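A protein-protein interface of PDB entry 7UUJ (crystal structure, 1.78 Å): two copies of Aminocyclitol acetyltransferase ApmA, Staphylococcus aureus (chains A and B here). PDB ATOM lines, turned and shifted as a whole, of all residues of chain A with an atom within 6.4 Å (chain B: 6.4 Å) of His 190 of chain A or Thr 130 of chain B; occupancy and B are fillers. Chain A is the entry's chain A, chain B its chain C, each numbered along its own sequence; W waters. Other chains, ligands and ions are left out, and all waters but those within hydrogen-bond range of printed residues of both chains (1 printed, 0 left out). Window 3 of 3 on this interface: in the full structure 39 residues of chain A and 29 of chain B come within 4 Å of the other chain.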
ATOM      1  N   ASN A 128       1.803  19.769   0.217  1.00  0.00           N
ATOM      2  CA  ASN A 128       0.504  20.404  -0.021  1.00  0.00           C
ATOM      3  C   ASN A 128      -0.623  19.584   0.606  1.00  0.00           C
ATOM      4  O   ASN A 128      -0.588  18.340   0.635  1.00  0.00           O
ATOM      5  CB  ASN A 128       0.250  20.568  -1.530  1.00  0.00           C
ATOM      6  CG  ASN A 128      -1.074  21.260  -1.841  1.00  0.00           C
ATOM      7  OD1 ASN A 128      -2.130  20.615  -1.961  1.00  0.00           O
ATOM      8  ND2 ASN A 128      -1.024  22.585  -1.973  1.00  0.00           N
ATOM      9  N   THR A 130      -3.511  18.649  -0.166  1.00  0.00           N
ATOM     10  CA  THR A 130      -4.294  17.666  -0.913  1.00  0.00           C
ATOM     11  C   THR A 130      -3.472  16.456  -1.363  1.00  0.00           C
ATOM     12  O   THR A 130      -4.014  15.598  -2.063  1.00  0.00           O
ATOM     13  CB  THR A 130      -4.936  18.284  -2.157  1.00  0.00           C
ATOM     14  OG1 THR A 130      -3.925  18.865  -2.976  1.00  0.00           O
ATOM     15  CG2 THR A 130      -5.934  19.381  -1.767  1.00  0.00           C
ATOM     16  N   ALA A 131      -2.178  16.379  -1.022  1.00  0.00           N
ATOM     17  CA  ALA A 131      -1.388  15.186  -1.341  1.00  0.00           C
ATOM     18  C   ALA A 131      -1.959  13.958  -0.641  1.00  0.00           C
ATOM     19  O   ALA A 131      -2.509  14.055   0.456  1.00  0.00           O
ATOM     20  CB  ALA A 131       0.077  15.380  -0.929  1.00  0.00           C
ATOM     21  N   GLU A 132      -1.816  12.787  -1.270  1.00  0.00           N
ATOM     22  CA  GLU A 132      -2.374  11.546  -0.738  1.00  0.00           C
ATOM     23  C   GLU A 132      -1.339  10.432  -0.732  1.00  0.00           C
ATOM     24  O   GLU A 132      -0.503  10.340  -1.634  1.00  0.00           O
ATOM     25  CB  GLU A 132      -3.567  11.081  -1.557  1.00  0.00           C
ATOM     26  CG  GLU A 132      -4.678  12.078  -1.617  1.00  0.00           C
ATOM     27  CD  GLU A 132      -5.878  11.633  -0.828  1.00  0.00           C
ATOM     28  OE1 GLU A 132      -5.769  11.460   0.413  1.00  0.00           O
ATOM     29  OE2 GLU A 132      -6.911  11.380  -1.487  1.00  0.00           O
ATOM     30  N   GLY A 188       3.604  18.631  -4.235  1.00  0.00           N
ATOM     31  CA  GLY A 188       2.575  19.520  -4.726  1.00  0.00           C
ATOM     32  C   GLY A 188       1.164  18.944  -4.603  1.00  0.00           C
ATOM     33  O   GLY A 188       0.945  17.829  -4.137  1.00  0.00           O
ATOM     34  N   ALA A 189       0.204  19.758  -5.028  1.00  0.00           N
ATOM     35  CA  ALA A 189      -1.215  19.462  -4.893  1.00  0.00           C
ATOM     36  C   ALA A 189      -1.626  18.226  -5.690  1.00  0.00           C
ATOM     37  O   ALA A 189      -1.137  17.969  -6.797  1.00  0.00           O
ATOM     38  CB  ALA A 189      -2.021  20.677  -5.334  1.00  0.00           C
ATOM     39  N   HIS A 190      -2.530  17.441  -5.103  1.00  0.00           N
ATOM     40  CA  HIS A 190      -3.074  16.216  -5.704  1.00  0.00           C
ATOM     41  C   HIS A 190      -1.998  15.203  -6.047  1.00  0.00           C
ATOM     42  O   HIS A 190      -2.245  14.292  -6.843  1.00  0.00           O
ATOM     43  CB  HIS A 190      -3.901  16.498  -6.972  1.00  0.00           C
ATOM     44  CG  HIS A 190      -4.945  17.542  -6.782  1.00  0.00           C
ATOM     45  ND1 HIS A 190      -5.103  18.602  -7.652  1.00  0.00           N
ATOM     46  CD2 HIS A 190      -5.868  17.708  -5.806  1.00  0.00           C
ATOM     47  CE1 HIS A 190      -6.093  19.368  -7.228  1.00  0.00           C
ATOM     48  NE2 HIS A 190      -6.576  18.846  -6.110  1.00  0.00           N
ATOM     49  N   ALA A 191      -0.794  15.353  -5.498  1.00  0.00           N
ATOM     50  CA  ALA A 191       0.200  14.311  -5.667  1.00  0.00           C
ATOM     51  C   ALA A 191      -0.204  13.065  -4.895  1.00  0.00           C
ATOM     52  O   ALA A 191      -0.873  13.128  -3.856  1.00  0.00           O
ATOM     53  CB  ALA A 191       1.578  14.805  -5.206  1.00  0.00           C
ATOM     54  N   PHE A 192       0.211  11.918  -5.418  1.00  0.00           N
ATOM     55  CA  PHE A 192      -0.070  10.619  -4.832  1.00  0.00           C
ATOM     56  C   PHE A 192       1.213   9.820  -4.725  1.00  0.00           C
ATOM     57  O   PHE A 192       2.004   9.797  -5.667  1.00  0.00           O
ATOM     58  CB  PHE A 192      -1.101   9.858  -5.666  1.00  0.00           C
ATOM     59  CG  PHE A 192      -1.263   8.422  -5.260  1.00  0.00           C
ATOM     60  CD1 PHE A 192      -2.015   8.082  -4.145  1.00  0.00           C
ATOM     61  CD2 PHE A 192      -0.726   7.412  -6.017  1.00  0.00           C
ATOM     62  CE1 PHE A 192      -2.181   6.742  -3.779  1.00  0.00           C
ATOM     63  CE2 PHE A 192      -0.916   6.067  -5.676  1.00  0.00           C
ATOM     64  CZ  PHE A 192      -1.623   5.741  -4.546  1.00  0.00           C
ATOM     65  N   GLY A 208       5.969  16.897  -8.261  1.00  0.00           N
ATOM     66  CA  GLY A 208       5.137  17.879  -8.929  1.00  0.00           C
ATOM     67  C   GLY A 208       3.661  17.700  -8.644  1.00  0.00           C
ATOM     68  O   GLY A 208       3.199  16.650  -8.209  1.00  0.00           O
ATOM     69  N   SER A 209       2.911  18.775  -8.884  1.00  0.00           N
ATOM     70  CA  SER A 209       1.472  18.723  -8.740  1.00  0.00           C
ATOM     71  C   SER A 209       0.912  17.628  -9.643  1.00  0.00           C
ATOM     72  O   SER A 209       1.305  17.509 -10.805  1.00  0.00           O
ATOM     73  CB  SER A 209       0.864  20.082  -9.086  1.00  0.00           C
ATOM     74  OG  SER A 209       1.106  21.012  -8.041  1.00  0.00           O
ATOM     75  N   GLY A 210       0.051  16.785  -9.089  1.00  0.00           N
ATOM     76  CA  GLY A 210      -0.555  15.747  -9.895  1.00  0.00           C
ATOM     77  C   GLY A 210       0.299  14.522 -10.168  1.00  0.00           C
ATOM     78  O   GLY A 210      -0.201  13.591 -10.818  1.00  0.00           O
ATOM     79  N   ALA A 211       1.553  14.473  -9.696  1.00  0.00           N
ATOM     80  CA  ALA A 211       2.393  13.296  -9.934  1.00  0.00           C
ATOM     81  C   ALA A 211       1.887  12.068  -9.172  1.00  0.00           C
ATOM     82  O   ALA A 211       1.382  12.166  -8.048  1.00  0.00           O
ATOM     83  CB  ALA A 211       3.853  13.574  -9.545  1.00  0.00           C
ATOM     84  N   VAL A 212       2.057  10.903  -9.781  1.00  0.00           N
ATOM     85  CA  VAL A 212       1.672   9.628  -9.190  1.00  0.00           C
ATOM     86  C   VAL A 212       2.959   8.843  -8.972  1.00  0.00           C
ATOM     87  O   VAL A 212       3.511   8.270  -9.915  1.00  0.00           O
ATOM     88  CB  VAL A 212       0.683   8.864 -10.078  1.00  0.00           C
ATOM     89  CG1 VAL A 212       0.540   7.412  -9.625  1.00  0.00           C
ATOM     90  CG2 VAL A 212      -0.679   9.552 -10.118  1.00  0.00           C
ATOM     91  N   GLY B 106     -14.851  26.569  -4.894  1.00  0.00           N
ATOM     92  CA  GLY B 106     -14.697  25.942  -3.602  1.00  0.00           C
ATOM     93  C   GLY B 106     -13.494  26.452  -2.822  1.00  0.00           C
ATOM     94  O   GLY B 106     -12.916  27.493  -3.133  1.00  0.00           O
ATOM     95  N   ASP B 107     -13.126  25.680  -1.789  1.00  0.00           N
ATOM     96  CA  ASP B 107     -12.238  26.179  -0.730  1.00  0.00           C
ATOM     97  C   ASP B 107     -10.824  26.447  -1.220  1.00  0.00           C
ATOM     98  O   ASP B 107     -10.150  27.353  -0.711  1.00  0.00           O
ATOM     99  CB  ASP B 107     -12.180  25.191   0.434  1.00  0.00           C
ATOM    100  CG  ASP B 107     -13.461  25.137   1.218  1.00  0.00           C
ATOM    101  OD1 ASP B 107     -14.169  26.167   1.268  1.00  0.00           O
ATOM    102  OD2 ASP B 107     -13.752  24.070   1.807  1.00  0.00           O
ATOM    103  N   ILE B 127     -16.606  26.549 -11.208  1.00  0.00           N
ATOM    104  CA  ILE B 127     -15.330  25.962 -10.800  1.00  0.00           C
ATOM    105  C   ILE B 127     -15.624  24.857  -9.806  1.00  0.00           C
ATOM    106  O   ILE B 127     -16.145  25.119  -8.723  1.00  0.00           O
ATOM    107  CB  ILE B 127     -14.385  27.019 -10.207  1.00  0.00           C
ATOM    108  CG1 ILE B 127     -14.203  28.167 -11.204  1.00  0.00           C
ATOM    109  CG2 ILE B 127     -13.040  26.375  -9.865  1.00  0.00           C
ATOM    110  CD1 ILE B 127     -13.354  29.377 -10.650  1.00  0.00           C
ATOM    111  N   ASN B 128     -15.309  23.626 -10.189  1.00  0.00           N
ATOM    112  CA  ASN B 128     -15.520  22.480  -9.319  1.00  0.00           C
ATOM    113  C   ASN B 128     -14.835  22.706  -7.982  1.00  0.00           C
ATOM    114  O   ASN B 128     -13.726  23.249  -7.914  1.00  0.00           O
ATOM    115  CB  ASN B 128     -14.968  21.210  -9.974  1.00  0.00           C
ATOM    116  CG  ASN B 128     -15.357  19.971  -9.231  1.00  0.00           C
ATOM    117  OD1 ASN B 128     -14.739  19.609  -8.220  1.00  0.00           O
ATOM    118  ND2 ASN B 128     -16.412  19.304  -9.708  1.00  0.00           N
ATOM    119  N   GLY B 129     -15.491  22.244  -6.915  1.00  0.00           N
ATOM    120  CA  GLY B 129     -14.999  22.522  -5.585  1.00  0.00           C
ATOM    121  C   GLY B 129     -13.632  21.934  -5.280  1.00  0.00           C
ATOM    122  O   GLY B 129     -12.989  22.387  -4.331  1.00  0.00           O
ATOM    123  N   THR B 130     -13.168  20.933  -6.039  1.00  0.00           N
ATOM    124  CA  THR B 130     -11.857  20.366  -5.740  1.00  0.00           C
ATOM    125  C   THR B 130     -10.725  20.950  -6.589  1.00  0.00           C
ATOM    126  O   THR B 130      -9.596  20.445  -6.518  1.00  0.00           O
ATOM    127  CB  THR B 130     -11.860  18.840  -5.908  1.00  0.00           C
ATOM    128  OG1 THR B 130     -12.213  18.492  -7.262  1.00  0.00           O
ATOM    129  CG2 THR B 130     -12.865  18.196  -4.937  1.00  0.00           C
ATOM    130  N   ALA B 131     -10.996  21.949  -7.408  1.00  0.00           N
ATOM    131  CA  ALA B 131      -9.939  22.618  -8.156  1.00  0.00           C
ATOM    132  C   ALA B 131      -9.003  23.348  -7.198  1.00  0.00           C
ATOM    133  O   ALA B 131      -9.418  23.854  -6.145  1.00  0.00           O
ATOM    134  CB  ALA B 131     -10.521  23.619  -9.148  1.00  0.00           C
ATOM    135  N   GLU B 132      -7.729  23.424  -7.581  1.00  0.00           N
ATOM    136  CA  GLU B 132      -6.725  24.005  -6.711  1.00  0.00           C
ATOM    137  C   GLU B 132      -5.877  24.989  -7.497  1.00  0.00           C
ATOM    138  O   GLU B 132      -5.576  24.772  -8.670  1.00  0.00           O
ATOM    139  CB  GLU B 132      -5.840  22.941  -6.084  1.00  0.00           C
ATOM    140  CG  GLU B 132      -6.568  21.959  -5.174  1.00  0.00           C
ATOM    141  CD  GLU B 132      -6.965  22.565  -3.825  1.00  0.00           C
ATOM    142  OE1 GLU B 132      -6.254  23.482  -3.332  1.00  0.00           O
ATOM    143  OE2 GLU B 132      -8.018  22.149  -3.281  1.00  0.00           O
ATOM    144  N   GLY B 188     -12.847  21.760 -14.108  1.00  0.00           N
ATOM    145  CA  GLY B 188     -13.306  20.457 -13.662  1.00  0.00           C
ATOM    146  C   GLY B 188     -12.702  20.018 -12.342  1.00  0.00           C
ATOM    147  O   GLY B 188     -11.845  20.669 -11.767  1.00  0.00           O
ATOM    148  N   ALA B 189     -13.147  18.853 -11.880  1.00  0.00           N
ATOM    149  CA  ALA B 189     -12.657  18.278 -10.626  1.00  0.00           C
ATOM    150  C   ALA B 189     -11.155  18.019 -10.672  1.00  0.00           C
ATOM    151  O   ALA B 189     -10.601  17.614 -11.699  1.00  0.00           O
ATOM    152  CB  ALA B 189     -13.390  16.960 -10.331  1.00  0.00           C
ATOM    153  N   HIS B 190     -10.498  18.258  -9.531  1.00  0.00           N
ATOM    154  CA  HIS B 190      -9.084  17.963  -9.303  1.00  0.00           C
ATOM    155  C   HIS B 190      -8.181  18.686 -10.275  1.00  0.00           C
ATOM    156  O   HIS B 190      -7.048  18.253 -10.495  1.00  0.00           O
ATOM    157  CB  HIS B 190      -8.782  16.455  -9.377  1.00  0.00           C
ATOM    158  CG  HIS B 190      -9.736  15.597  -8.609  1.00  0.00           C
ATOM    159  ND1 HIS B 190     -10.105  15.870  -7.307  1.00  0.00           N
ATOM    160  CD2 HIS B 190     -10.417  14.482  -8.968  1.00  0.00           C
ATOM    161  CE1 HIS B 190     -10.951  14.941  -6.887  1.00  0.00           C
ATOM    162  NE2 HIS B 190     -11.165  14.094  -7.880  1.00  0.00           N
ATOM    163  N   ALA B 191      -8.666  19.749 -10.900  1.00  0.00           N
ATOM    164  CA  ALA B 191      -7.815  20.517 -11.789  1.00  0.00           C
ATOM    165  C   ALA B 191      -6.870  21.376 -10.952  1.00  0.00           C
ATOM    166  O   ALA B 191      -7.142  21.698  -9.795  1.00  0.00           O
ATOM    167  CB  ALA B 191      -8.669  21.377 -12.716  1.00  0.00           C
ATOM    168  N   PHE B 192      -5.710  21.684 -11.517  1.00  0.00           N
ATOM    169  CA  PHE B 192      -4.731  22.529 -10.856  1.00  0.00           C
ATOM    170  C   PHE B 192      -4.266  23.619 -11.809  1.00  0.00           C
ATOM    171  O   PHE B 192      -3.998  23.344 -12.982  1.00  0.00           O
ATOM    172  CB  PHE B 192      -3.539  21.710 -10.378  1.00  0.00           C
ATOM    173  CG  PHE B 192      -2.404  22.541  -9.944  1.00  0.00           C
ATOM    174  CD1 PHE B 192      -2.425  23.187  -8.716  1.00  0.00           C
ATOM    175  CD2 PHE B 192      -1.288  22.691 -10.765  1.00  0.00           C
ATOM    176  CE1 PHE B 192      -1.353  23.983  -8.328  1.00  0.00           C
ATOM    177  CE2 PHE B 192      -0.222  23.484 -10.367  1.00  0.00           C
ATOM    178  CZ  PHE B 192      -0.266  24.129  -9.162  1.00  0.00           C
HETATM  179  O   HOH W   1      -8.631  19.656  -4.106  1.00  0.00           O
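A ring nitrogen (NE2) of His 190 of chain A lies within hydrogen-bond range of the backbone carbonyl oxygen (O) of Thr 130 of chain B (3.4 Å).
A ring nitrogen (ND1) of His 190 of chain A sits at hydrogen-bond distance from the backbone carbonyl oxygen (O) of His 190 of chain B, at 3.5 Å.
Glu 132 of chain B touches Thr 130 of chain A (OE2 to CG2, 3.8 Å).
His 190 of chain A touches Glu 132 of chain B.
CE1 of His 190 of chain A touches O of Ala 191 of chain B, 3.6 Å away.
CZ of Phe 192 of chain B touches OG of Ser 209 of chain A, at 3.6 Å.
Water W1 lies within hydrogen-bond range of the side-chain carboxylate (OE2) of Glu 132 of chain B (2.7 Å), the backbone carbonyl oxygen (O) of Thr 130 of chain B (2.7 Å) and a ring nitrogen (NE2) of His 190 of chain A (3.0 Å).
Thr 130 of chain A touches Glu 132 of chain B, but with the chains exchanged Glu 132 of chain A does not touch Thr 130 of chain B (9.7 Å).
His 190 of chain A touches Thr 130 of chain B, but with the chains exchanged Thr 130 of chain A does not touch His 190 of chain B (7.7 Å).
His 190 of chain A touches its own counterpart, His 190 of chain B.
His 190 of chain A touches Ala 191 of chain B, but with the chains exchanged Ala 191 of chain A does not touch His 190 of chain B (8.5 Å).
Positions printed for both chains: 128, 130, 131, 132, 188, 189, 190, 191 and 192.
Of the 6 pairs that touch across the chains among the printed residues, 1 has its exchanged pair printed and touching as well.
Printed residues of chain A that touch a printed residue of chain B: Thr 130, His 190 and Ser 209.
OD1 of Asn 128 of chain A lies within hydrogen-bond range of OG1 of Thr 130 of chain A, 2.7 Å away.
The side-chain hydroxyl (OG1) of Thr 130 of chain A is in hydrogen-bond range of the backbone NH (N) of His 190 of chain A.
The side-chain hydroxyl of Ser 209 of chain A sits at hydrogen-bond distance from the backbone NH of Ala 189 of chain A (3.4 Å).
The side-chain amide oxygen of Asn 128 of chain B is in hydrogen-bond range of the side-chain hydroxyl of Thr 130 of chain B (2.9 Å).
N of His 190 of chain B lies within hydrogen-bond range of OG1 of Thr 130 of chain B (2.9 Å).
O of Ala 191 of chain B is in hydrogen-bond range of N of Glu 132 of chain B (2.9 Å).
Asn 128 of chain A touches none of the printed residues of chain B.
Of the printed residues of chain B, Thr 130 of chain A touches Glu 132.
His 190 of chain A touches just these residues of chain B: Thr 130 (3.4 Å), Glu 132 (3.3 Å), His 190 (3.5 Å) and Ala 191 (3.6 Å).
Of the printed residues of chain B, Ser 209 of chain A touches Phe 192 (3.6 Å).
Gly 106 of chain B touches none of the printed residues of chain A.
Of chain A, only His 190 (3.4 Å) comes within 4 Å of Thr 130 of chain B.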
